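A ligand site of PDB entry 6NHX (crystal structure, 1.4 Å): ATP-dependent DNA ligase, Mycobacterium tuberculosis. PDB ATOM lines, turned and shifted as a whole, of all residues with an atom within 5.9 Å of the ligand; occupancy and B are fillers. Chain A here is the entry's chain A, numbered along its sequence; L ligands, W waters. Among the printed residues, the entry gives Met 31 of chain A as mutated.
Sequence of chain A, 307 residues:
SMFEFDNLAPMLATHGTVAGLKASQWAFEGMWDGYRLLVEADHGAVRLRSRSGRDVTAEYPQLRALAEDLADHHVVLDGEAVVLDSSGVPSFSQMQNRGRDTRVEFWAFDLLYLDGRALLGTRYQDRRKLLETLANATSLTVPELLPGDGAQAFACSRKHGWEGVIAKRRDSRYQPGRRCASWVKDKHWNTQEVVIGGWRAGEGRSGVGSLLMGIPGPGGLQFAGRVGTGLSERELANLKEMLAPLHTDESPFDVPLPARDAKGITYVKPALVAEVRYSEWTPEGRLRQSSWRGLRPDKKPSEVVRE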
ATOM      1  N   MET A  11       3.025 -37.621  16.800  1.00  0.00           N
ATOM      2  CA  MET A  11       4.312 -36.949  16.924  1.00  0.00           C
ATOM      3  C   MET A  11       4.144 -35.483  16.532  1.00  0.00           C
ATOM      4  O   MET A  11       3.310 -35.129  15.690  1.00  0.00           O
ATOM      5  CB  MET A  11       5.273 -37.628  15.949  1.00  0.00           C
ATOM      6  CG  MET A  11       6.713 -37.146  16.035  1.00  0.00           C
ATOM      7  SD  MET A  11       7.766 -38.191  15.002  1.00  0.00           S
ATOM      8  CE  MET A  11       9.335 -37.322  15.171  1.00  0.00           C
ATOM      9  N   LEU A  12       4.945 -34.618  17.145  1.00  0.00           N
ATOM     10  CA  LEU A  12       4.793 -33.170  16.985  1.00  0.00           C
ATOM     11  C   LEU A  12       6.108 -32.553  16.504  1.00  0.00           C
ATOM     12  O   LEU A  12       7.186 -33.102  16.720  1.00  0.00           O
ATOM     13  CB  LEU A  12       4.324 -32.526  18.287  1.00  0.00           C
ATOM     14  CG  LEU A  12       2.982 -33.050  18.803  1.00  0.00           C
ATOM     15  CD1 LEU A  12       2.712 -32.517  20.210  1.00  0.00           C
ATOM     16  CD2 LEU A  12       1.838 -32.672  17.855  1.00  0.00           C
ATOM     17  N   ALA A  13       5.978 -31.387  15.854  1.00  0.00           N
ATOM     18  CA  ALA A  13       7.101 -30.682  15.240  1.00  0.00           C
ATOM     19  C   ALA A  13       7.543 -29.517  16.105  1.00  0.00           C
ATOM     20  O   ALA A  13       6.767 -28.944  16.872  1.00  0.00           O
ATOM     21  CB  ALA A  13       6.723 -30.137  13.851  1.00  0.00           C
ATOM     22  N   GLU A  29       7.640 -31.365   3.516  1.00  0.00           N
ATOM     23  CA  GLU A  29       6.222 -31.503   3.242  1.00  0.00           C
ATOM     24  C   GLU A  29       5.539 -30.151   3.358  1.00  0.00           C
ATOM     25  O   GLU A  29       5.997 -29.283   4.117  1.00  0.00           O
ATOM     26  CB  GLU A  29       5.578 -32.437   4.273  1.00  0.00           C
ATOM     27  CG  GLU A  29       5.988 -33.902   4.193  1.00  0.00           C
ATOM     28  CD  GLU A  29       5.210 -34.773   5.167  1.00  0.00           C
ATOM     29  OE1 GLU A  29       5.761 -35.792   5.599  1.00  0.00           O
ATOM     30  OE2 GLU A  29       4.064 -34.417   5.512  1.00  0.00           O
ATOM     31  N   GLY A  30       4.438 -29.980   2.655  1.00  0.00           N
ATOM     32  CA  GLY A  30       3.583 -28.845   2.915  1.00  0.00           C
ATOM     33  C   GLY A  30       2.954 -28.921   4.293  1.00  0.00           C
ATOM     34  O   GLY A  30       2.662 -30.003   4.824  1.00  0.00           O
ATOM     35  N   MET A  31       2.793 -27.759   4.913  1.00  0.00           N
ATOM     36  CA  MET A  31       2.044 -27.640   6.160  1.00  0.00           C
ATOM     37  C   MET A  31       0.567 -27.439   5.822  1.00  0.00           C
ATOM     38  O   MET A  31       0.213 -26.448   5.170  1.00  0.00           O
ATOM     39  CB  MET A  31       2.559 -26.471   6.987  1.00  0.00           C
ATOM     40  CG  MET A  31       1.737 -26.243   8.257  1.00  0.00           C
ATOM     41  SD  MET A  31       2.179 -24.716   9.101  1.00  0.00           S
ATOM     42  CE  MET A  31       3.828 -25.134   9.686  1.00  0.00           C
ATOM     43  N   TRP A  32      -0.282 -28.359   6.292  1.00  0.00           N
ATOM     44  CA  TRP A  32      -1.712 -28.372   5.991  1.00  0.00           C
ATOM     45  C   TRP A  32      -2.512 -27.932   7.216  1.00  0.00           C
ATOM     46  O   TRP A  32      -2.479 -28.610   8.250  1.00  0.00           O
ATOM     47  CB  TRP A  32      -2.171 -29.772   5.555  1.00  0.00           C
ATOM     48  CG  TRP A  32      -1.231 -30.445   4.587  1.00  0.00           C
ATOM     49  CD1 TRP A  32      -0.613 -31.669   4.753  1.00  0.00           C
ATOM     50  CD2 TRP A  32      -0.788 -29.936   3.328  1.00  0.00           C
ATOM     51  NE1 TRP A  32       0.179 -31.944   3.656  1.00  0.00           N
ATOM     52  CE2 TRP A  32       0.106 -30.888   2.781  1.00  0.00           C
ATOM     53  CE3 TRP A  32      -1.025 -28.747   2.622  1.00  0.00           C
ATOM     54  CZ2 TRP A  32       0.723 -30.705   1.540  1.00  0.00           C
ATOM     55  CZ3 TRP A  32      -0.399 -28.561   1.393  1.00  0.00           C
ATOM     56  CH2 TRP A  32       0.458 -29.545   0.861  1.00  0.00           C
ATOM     57  N   ASP A  33      -3.238 -26.805   7.118  1.00  0.00           N
ATOM     58  CA  ASP A  33      -4.094 -26.386   8.218  1.00  0.00           C
ATOM     59  C   ASP A  33      -5.331 -27.281   8.283  1.00  0.00           C
ATOM     60  O   ASP A  33      -6.073 -27.392   7.299  1.00  0.00           O
ATOM     61  CB  ASP A  33      -4.526 -24.932   8.057  1.00  0.00           C
ATOM     62  CG  ASP A  33      -3.569 -23.952   8.714  1.00  0.00           C
ATOM     63  OD1 ASP A  33      -2.415 -24.341   8.985  1.00  0.00           O
ATOM     64  OD2 ASP A  33      -3.952 -22.778   8.965  1.00  0.00           O
ATOM     65  N   GLY A  34      -5.551 -27.930   9.417  1.00  0.00           N
ATOM     66  CA  GLY A  34      -6.695 -28.797   9.586  1.00  0.00           C
ATOM     67  C   GLY A  34      -6.679 -29.378  10.996  1.00  0.00           C
ATOM     68  O   GLY A  34      -6.122 -28.747  11.908  1.00  0.00           O
ATOM     69  N   ARG A  36      -5.472 -32.770  13.191  1.00  0.00           N
ATOM     70  CA  ARG A  36      -4.629 -33.947  13.144  1.00  0.00           C
ATOM     71  C   ARG A  36      -5.436 -35.193  13.491  1.00  0.00           C
ATOM     72  O   ARG A  36      -6.180 -35.213  14.476  1.00  0.00           O
ATOM     73  CB  ARG A  36      -3.496 -33.787  14.163  1.00  0.00           C
ATOM     74  CG  ARG A  36      -2.453 -34.872  14.084  1.00  0.00           C
ATOM     75  CD  ARG A  36      -1.535 -34.666  12.905  1.00  0.00           C
ATOM     76  NE  ARG A  36      -0.380 -35.548  12.946  1.00  0.00           N
ATOM     77  CZ  ARG A  36       0.746 -35.286  13.599  1.00  0.00           C
ATOM     78  NH1 ARG A  36       0.887 -34.146  14.268  1.00  0.00           N
ATOM     79  NH2 ARG A  36       1.742 -36.157  13.581  1.00  0.00           N
ATOM     80  N   ARG A  51      -5.820 -35.486  18.214  1.00  0.00           N
ATOM     81  CA  ARG A  51      -4.527 -35.185  18.822  1.00  0.00           C
ATOM     82  C   ARG A  51      -4.555 -35.414  20.335  1.00  0.00           C
ATOM     83  O   ARG A  51      -3.544 -35.792  20.929  1.00  0.00           O
ATOM     84  CB  ARG A  51      -4.115 -33.751  18.492  1.00  0.00           C
ATOM     85  CG  ARG A  51      -2.740 -33.374  18.982  1.00  0.00           C
ATOM     86  CD  ARG A  51      -2.881 -32.269  19.971  1.00  0.00           C
ATOM     87  NE  ARG A  51      -1.614 -31.691  20.410  1.00  0.00           N
ATOM     88  CZ  ARG A  51      -0.894 -30.827  19.705  1.00  0.00           C
ATOM     89  NH1 ARG A  51      -1.288 -30.434  18.503  1.00  0.00           N
ATOM     90  NH2 ARG A  51       0.211 -30.328  20.225  1.00  0.00           N
ATOM     91  N   GLU A  80      -3.834 -35.298   8.222  1.00  0.00           N
ATOM     92  CA  GLU A  80      -4.647 -34.139   8.571  1.00  0.00           C
ATOM     93  C   GLU A  80      -6.005 -34.264   7.916  1.00  0.00           C
ATOM     94  O   GLU A  80      -6.095 -34.534   6.723  1.00  0.00           O
ATOM     95  CB  GLU A  80      -3.969 -32.853   8.057  1.00  0.00           C
ATOM     96  CG  GLU A  80      -4.409 -31.587   8.778  1.00  0.00           C
ATOM     97  CD  GLU A  80      -3.498 -31.249   9.942  1.00  0.00           C
ATOM     98  OE1 GLU A  80      -2.526 -31.991  10.176  1.00  0.00           O
ATOM     99  OE2 GLU A  80      -3.755 -30.240  10.630  1.00  0.00           O
ATOM    100  N   PHE A 109       0.124 -38.385   5.770  1.00  0.00           N
ATOM    101  CA  PHE A 109       1.543 -38.097   5.656  1.00  0.00           C
ATOM    102  C   PHE A 109       2.448 -39.047   6.436  1.00  0.00           C
ATOM    103  O   PHE A 109       3.676 -38.898   6.380  1.00  0.00           O
ATOM    104  CB  PHE A 109       1.888 -36.623   5.963  1.00  0.00           C
ATOM    105  CG  PHE A 109       1.282 -36.072   7.230  1.00  0.00           C
ATOM    106  CD1 PHE A 109       1.622 -36.580   8.490  1.00  0.00           C
ATOM    107  CD2 PHE A 109       0.410 -34.954   7.173  1.00  0.00           C
ATOM    108  CE1 PHE A 109       1.079 -36.044   9.657  1.00  0.00           C
ATOM    109  CE2 PHE A 109      -0.133 -34.418   8.341  1.00  0.00           C
ATOM    110  CZ  PHE A 109       0.201 -34.957   9.574  1.00  0.00           C
ATOM    111  N   ILE A 166       6.732 -28.464   6.758  1.00  0.00           N
ATOM    112  CA  ILE A 166       7.264 -29.327   7.811  1.00  0.00           C
ATOM    113  C   ILE A 166       8.453 -30.052   7.213  1.00  0.00           C
ATOM    114  O   ILE A 166       8.287 -30.831   6.263  1.00  0.00           O
ATOM    115  CB  ILE A 166       6.250 -30.347   8.358  1.00  0.00           C
ATOM    116  CG1 ILE A 166       4.849 -29.737   8.479  1.00  0.00           C
ATOM    117  CG2 ILE A 166       6.794 -30.954   9.681  1.00  0.00           C
ATOM    118  CD1 ILE A 166       4.699 -28.833   9.663  1.00  0.00           C
ATOM    119  N   LYS A 168      11.142 -33.036   7.806  1.00  0.00           N
ATOM    120  CA  LYS A 168      11.244 -34.244   8.599  1.00  0.00           C
ATOM    121  C   LYS A 168      12.537 -34.966   8.235  1.00  0.00           C
ATOM    122  O   LYS A 168      12.827 -35.161   7.046  1.00  0.00           O
ATOM    123  CB  LYS A 168      10.016 -35.138   8.380  1.00  0.00           C
ATOM    124  CG  LYS A 168       8.733 -34.428   8.773  1.00  0.00           C
ATOM    125  CD  LYS A 168       7.487 -35.241   8.404  1.00  0.00           C
ATOM    126  CE  LYS A 168       6.211 -34.517   8.790  1.00  0.00           C
ATOM    127  NZ  LYS A 168       5.008 -35.290   8.329  1.00  0.00           N
ATOM    128  N   ARG A 179       7.107 -34.042  20.992  1.00  0.00           N
ATOM    129  CA  ARG A 179       7.576 -33.015  20.082  1.00  0.00           C
ATOM    130  C   ARG A 179       9.082 -33.170  19.935  1.00  0.00           C
ATOM    131  O   ARG A 179       9.797 -33.231  20.927  1.00  0.00           O
ATOM    132  CB  ARG A 179       7.232 -31.625  20.623  1.00  0.00           C
ATOM    133  CG  ARG A 179       7.391 -30.526  19.591  1.00  0.00           C
ATOM    134  CD  ARG A 179       7.025 -29.150  20.169  1.00  0.00           C
ATOM    135  NE  ARG A 179       5.651 -29.113  20.697  1.00  0.00           N
ATOM    136  CZ  ARG A 179       4.570 -28.850  19.975  1.00  0.00           C
ATOM    137  NH1 ARG A 179       4.668 -28.607  18.667  1.00  0.00           N
ATOM    138  NH2 ARG A 179       3.379 -28.807  20.577  1.00  0.00           N
ATOM    139  N   TRP A 183      11.506 -33.090  13.509  1.00  0.00           N
ATOM    140  CA  TRP A 183      10.463 -32.481  12.702  1.00  0.00           C
ATOM    141  C   TRP A 183      10.474 -30.987  12.985  1.00  0.00           C
ATOM    142  O   TRP A 183      10.424 -30.581  14.150  1.00  0.00           O
ATOM    143  CB  TRP A 183       9.075 -33.003  13.093  1.00  0.00           C
ATOM    144  CG  TRP A 183       8.669 -34.373  12.612  1.00  0.00           C
ATOM    145  CD1 TRP A 183       9.486 -35.373  12.193  1.00  0.00           C
ATOM    146  CD2 TRP A 183       7.338 -34.855  12.505  1.00  0.00           C
ATOM    147  NE1 TRP A 183       8.729 -36.479  11.840  1.00  0.00           N
ATOM    148  CE2 TRP A 183       7.408 -36.178  12.021  1.00  0.00           C
ATOM    149  CE3 TRP A 183       6.084 -34.300  12.782  1.00  0.00           C
ATOM    150  CZ2 TRP A 183       6.252 -36.952  11.802  1.00  0.00           C
ATOM    151  CZ3 TRP A 183       4.951 -35.058  12.560  1.00  0.00           C
ATOM    152  CH2 TRP A 183       5.049 -36.371  12.081  1.00  0.00           C
ATOM    153  N   LYS A 185       8.757 -27.220  11.962  1.00  0.00           N
ATOM    154  CA  LYS A 185       7.627 -26.549  11.322  1.00  0.00           C
ATOM    155  C   LYS A 185       7.930 -25.064  11.149  1.00  0.00           C
ATOM    156  O   LYS A 185       8.495 -24.434  12.037  1.00  0.00           O
ATOM    157  CB  LYS A 185       6.330 -26.729  12.124  1.00  0.00           C
ATOM    158  CG  LYS A 185       6.457 -26.449  13.611  1.00  0.00           C
ATOM    159  CD  LYS A 185       5.086 -26.388  14.276  1.00  0.00           C
ATOM    160  CE  LYS A 185       5.208 -25.969  15.729  1.00  0.00           C
ATOM    161  NZ  LYS A 185       3.871 -25.688  16.347  1.00  0.00           N
ATOM    162  N   LYS A 187       6.302 -21.421   9.072  1.00  0.00           N
ATOM    163  CA  LYS A 187       5.203 -20.781   8.357  1.00  0.00           C
ATOM    164  C   LYS A 187       5.696 -19.556   7.600  1.00  0.00           C
ATOM    165  O   LYS A 187       6.615 -18.871   8.049  1.00  0.00           O
ATOM    166  CB  LYS A 187       4.104 -20.363   9.339  1.00  0.00           C
ATOM    167  CG  LYS A 187       3.437 -21.527  10.053  1.00  0.00           C
ATOM    168  CD  LYS A 187       2.075 -21.133  10.594  1.00  0.00           C
ATOM    169  CE  LYS A 187       1.758 -21.858  11.876  1.00  0.00           C
ATOM    170  NZ  LYS A 187       2.057 -21.030  13.067  1.00  0.00           N
ATOM    171  N   GLU A 275      -6.053 -16.802  16.447  1.00  0.00           N
ATOM    172  CA  GLU A 275      -4.763 -16.602  15.835  1.00  0.00           C
ATOM    173  C   GLU A 275      -4.947 -15.813  14.544  1.00  0.00           C
ATOM    174  O   GLU A 275      -5.854 -16.108  13.764  1.00  0.00           O
ATOM    175  CB  GLU A 275      -4.095 -17.934  15.522  1.00  0.00           C
ATOM    176  CG  GLU A 275      -2.937 -18.250  16.424  1.00  0.00           C
ATOM    177  CD  GLU A 275      -2.340 -19.600  16.132  1.00  0.00           C
ATOM    178  OE1 GLU A 275      -1.255 -19.905  16.678  1.00  0.00           O
ATOM    179  OE2 GLU A 275      -2.958 -20.375  15.366  1.00  0.00           O
ATOM    180  N   ARG A 293      -6.726 -16.606  10.988  1.00  0.00           N
ATOM    181  CA  ARG A 293      -6.475 -18.043  10.901  1.00  0.00           C
ATOM    182  C   ARG A 293      -7.619 -18.843  11.500  1.00  0.00           C
ATOM    183  O   ARG A 293      -8.170 -19.726  10.832  1.00  0.00           O
ATOM    184  CB  ARG A 293      -5.123 -18.428  11.494  1.00  0.00           C
ATOM    185  CG  ARG A 293      -4.606 -19.765  10.984  1.00  0.00           C
ATOM    186  CD  ARG A 293      -3.531 -20.323  11.884  1.00  0.00           C
ATOM    187  NE  ARG A 293      -2.888 -21.491  11.299  1.00  0.00           N
ATOM    188  CZ  ARG A 293      -1.966 -22.224  11.911  1.00  0.00           C
ATOM    189  NH1 ARG A 293      -1.583 -21.912  13.142  1.00  0.00           N
ATOM    190  NH2 ARG A 293      -1.429 -23.269  11.291  1.00  0.00           N
ATOM    191  N   ARG A 296      -8.703 -20.393  18.675  1.00  0.00           N
ATOM    192  CA  ARG A 296      -7.831 -21.330  19.379  1.00  0.00           C
ATOM    193  C   ARG A 296      -8.505 -21.683  20.705  1.00  0.00           C
ATOM    194  O   ARG A 296      -8.179 -21.112  21.757  1.00  0.00           O
ATOM    195  CB  ARG A 296      -6.430 -20.749  19.598  1.00  0.00           C
ATOM    196  CG  ARG A 296      -5.617 -20.466  18.320  1.00  0.00           C
ATOM    197  CD  ARG A 296      -5.762 -21.563  17.271  1.00  0.00           C
ATOM    198  NE  ARG A 296      -5.297 -22.864  17.727  1.00  0.00           N
ATOM    199  CZ  ARG A 296      -4.120 -23.401  17.400  1.00  0.00           C
ATOM    200  NH1 ARG A 296      -3.276 -22.738  16.619  1.00  0.00           N
ATOM    201  NH2 ARG A 296      -3.778 -24.598  17.865  1.00  0.00           N
ATOM    202  N   LYS A 299      -6.484 -22.329  24.045  1.00  0.00           N
ATOM    203  CA  LYS A 299      -5.562 -21.340  24.558  1.00  0.00           C
ATOM    204  C   LYS A 299      -6.289 -20.415  25.518  1.00  0.00           C
ATOM    205  O   LYS A 299      -7.490 -20.143  25.362  1.00  0.00           O
ATOM    206  CB  LYS A 299      -4.936 -20.544  23.416  1.00  0.00           C
ATOM    207  CG  LYS A 299      -4.086 -21.439  22.537  1.00  0.00           C
ATOM    208  CD  LYS A 299      -3.166 -20.667  21.612  1.00  0.00           C
ATOM    209  CE  LYS A 299      -2.242 -21.638  20.874  1.00  0.00           C
ATOM    210  NZ  LYS A 299      -1.321 -20.929  19.948  1.00  0.00           N
HETATM  211  P1  LIG L   1       1.031 -27.743  17.599  1.00  0.00           P
HETATM  212  O1  LIG L   1       2.376 -27.990  16.943  1.00  0.00           O
HETATM  213  O2  LIG L   1       1.012 -27.886  19.111  1.00  0.00           O
HETATM  214  O3  LIG L   1      -0.087 -28.518  16.921  1.00  0.00           O
HETATM  215  P2  LIG L   1      -0.285 -25.445  16.353  1.00  0.00           P
HETATM  216  O4  LIG L   1      -0.242 -23.966  16.595  1.00  0.00           O
HETATM  217  O5  LIG L   1      -1.601 -26.194  16.271  1.00  0.00           O
HETATM  218  O6  LIG L   1       0.715 -26.162  17.395  1.00  0.00           O
HETATM  219  P3  LIG L   1       1.275 -24.836  13.974  1.00  0.00           P
HETATM  220  O7  LIG L   1       2.347 -24.110  14.721  1.00  0.00           O
HETATM  221  O8  LIG L   1       0.203 -24.174  13.147  1.00  0.00           O
HETATM  222  O9  LIG L   1       0.532 -25.799  15.023  1.00  0.00           O
HETATM  223  O10 LIG L   1       1.948 -26.075  13.178  1.00  0.00           O
HETATM  224  C1  LIG L   1       1.216 -26.777  12.168  1.00  0.00           C
HETATM  225  C2  LIG L   1       0.317 -27.853  12.796  1.00  0.00           C
HETATM  226  O11 LIG L   1      -0.198 -28.641  11.720  1.00  0.00           O
HETATM  227  C3  LIG L   1       1.064 -28.806  13.715  1.00  0.00           C
HETATM  228  O12 LIG L   1       0.124 -29.390  14.620  1.00  0.00           O
HETATM  229  C4  LIG L   1       1.501 -29.864  12.734  1.00  0.00           C
HETATM  230  O13 LIG L   1       1.785 -31.118  13.368  1.00  0.00           O
HETATM  231  C5  LIG L   1       0.299 -29.974  11.807  1.00  0.00           C
HETATM  232  N1  LIG L   1       0.695 -30.324  10.423  1.00  0.00           N
HETATM  233  C6  LIG L   1       0.246 -29.731   9.288  1.00  0.00           C
HETATM  234  N2  LIG L   1       0.788 -30.319   8.183  1.00  0.00           N
HETATM  235  C7  LIG L   1       1.585 -31.315   8.639  1.00  0.00           C
HETATM  236  C8  LIG L   1       2.446 -32.305   8.015  1.00  0.00           C
HETATM  237  N3  LIG L   1       2.597 -32.330   6.685  1.00  0.00           N
HETATM  238  N4  LIG L   1       3.102 -33.153   8.819  1.00  0.00           N
HETATM  239  C9  LIG L   1       2.977 -33.140  10.149  1.00  0.00           C
HETATM  240  N5  LIG L   1       2.210 -32.248  10.794  1.00  0.00           N
HETATM  241  C10 LIG L   1       1.515 -31.317  10.090  1.00  0.00           C
HETATM  242  O   HOH W   1       3.401 -30.219  15.502  1.00  0.00           O
HETATM  243  O   HOH W   2       0.257 -23.463  19.476  1.00  0.00           O
HETATM  244  O   HOH W   3      -1.521 -26.927  20.169  1.00  0.00           O
HETATM  245  O   HOH W   4      -0.749 -31.999  14.962  1.00  0.00           O
HETATM  246  O   HOH W   5       0.457 -21.608  15.624  1.00  0.00           O
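Met 31 touches the ligand.
Glu 80 touches the ligand (OE1 to N1, 3.6 Å).
CE2 of Phe 109 touches C8 of the ligand, 3.3 Å away.
CG1 of Ile 166 touches C8 of the ligand, 3.5 Å away.
Trp 183 touches the ligand.
The nearest printed residue that does not touch the ligand is Glu 275 (4.2 Å).
The guanidinium group (NH1) of Arg 293 is in salt-bridge range of the side-chain carboxylate (OE2) of Glu 275 (3.0 Å).
The guanidinium group of Arg 293 lies within salt-bridge range of the side-chain carboxylate of Asp 33, at 2.7 Å.
The side-chain carboxylate of Glu 29 is in salt-bridge range of the side-chain amino group of Lys 168, at 2.9 Å.
O of Glu 29 is in hydrogen-bond range of N of Ile 166 (2.9 Å).
The guanidinium group (NH1) of Arg 179 sits at hydrogen-bond distance from the backbone carbonyl oxygen (O) of Ala 13 (2.8 Å).
OE2 of Glu 275 is in salt-bridge range of NH1 of Arg 296.
O of Met 11 sits at hydrogen-bond distance from NH2 of Arg 36.
The side-chain carboxylate (OE2) of Glu 80 sits close to the backbone NH (N) of Gly 34, at 3.2 Å.
Water W5 lies within hydrogen-bond range of OE1 of Glu 275, O4 of the ligand, NZ of Lys 187 and NH1 of Arg 293.
Water W4 lies within hydrogen-bond range of an oxygen (O12) of the ligand and the guanidinium group (NH1) of Arg 36.
Water W1 bridges O13 of the ligand (2.8 Å) and N of Ala 13 (2.9 Å).
Water W2 bridges an oxygen (O4) of the ligand (3.0 Å) and the side-chain amino group (NZ) of Lys 299 (3.0 Å).
The guanidinium group (NH2) of Arg 293 lies within salt-bridge range of an oxygen (O8) of the ligand, at 2.6 Å.
NZ of Lys 185 is in salt-bridge range of O7 of the ligand (2.7 Å).
The guanidinium group (NH1) of Arg 51 lies within salt-bridge range of an oxygen (O3) of the ligand (2.8 Å).
N3 of the ligand is in hydrogen-bond range of OE2 of Glu 29 (2.8 Å).
The side-chain amino group (NZ) of Lys 168 sits at hydrogen-bond distance from a nitrogen (N4) of the ligand, 2.9 Å away.
N of Trp 32 lies within hydrogen-bond range of N2 of the ligand (2.9 Å).
NH2 of Arg 179 lies within salt-bridge range of O2 of the ligand.
A nitrogen (N3) of the ligand sits at hydrogen-bond distance from the backbone carbonyl oxygen (O) of Gly 30 (3.0 Å).
The side-chain amino group (NZ) of Lys 187 is in salt-bridge range of an oxygen (O7) of the ligand, at 3.5 Å.
The guanidinium group (NH2) of Arg 296 is in salt-bridge range of an oxygen (O5) of the ligand (3.1 Å).
The guanidinium group (NH1) of Arg 36 lies within hydrogen-bond range of an oxygen (O13) of the ligand.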
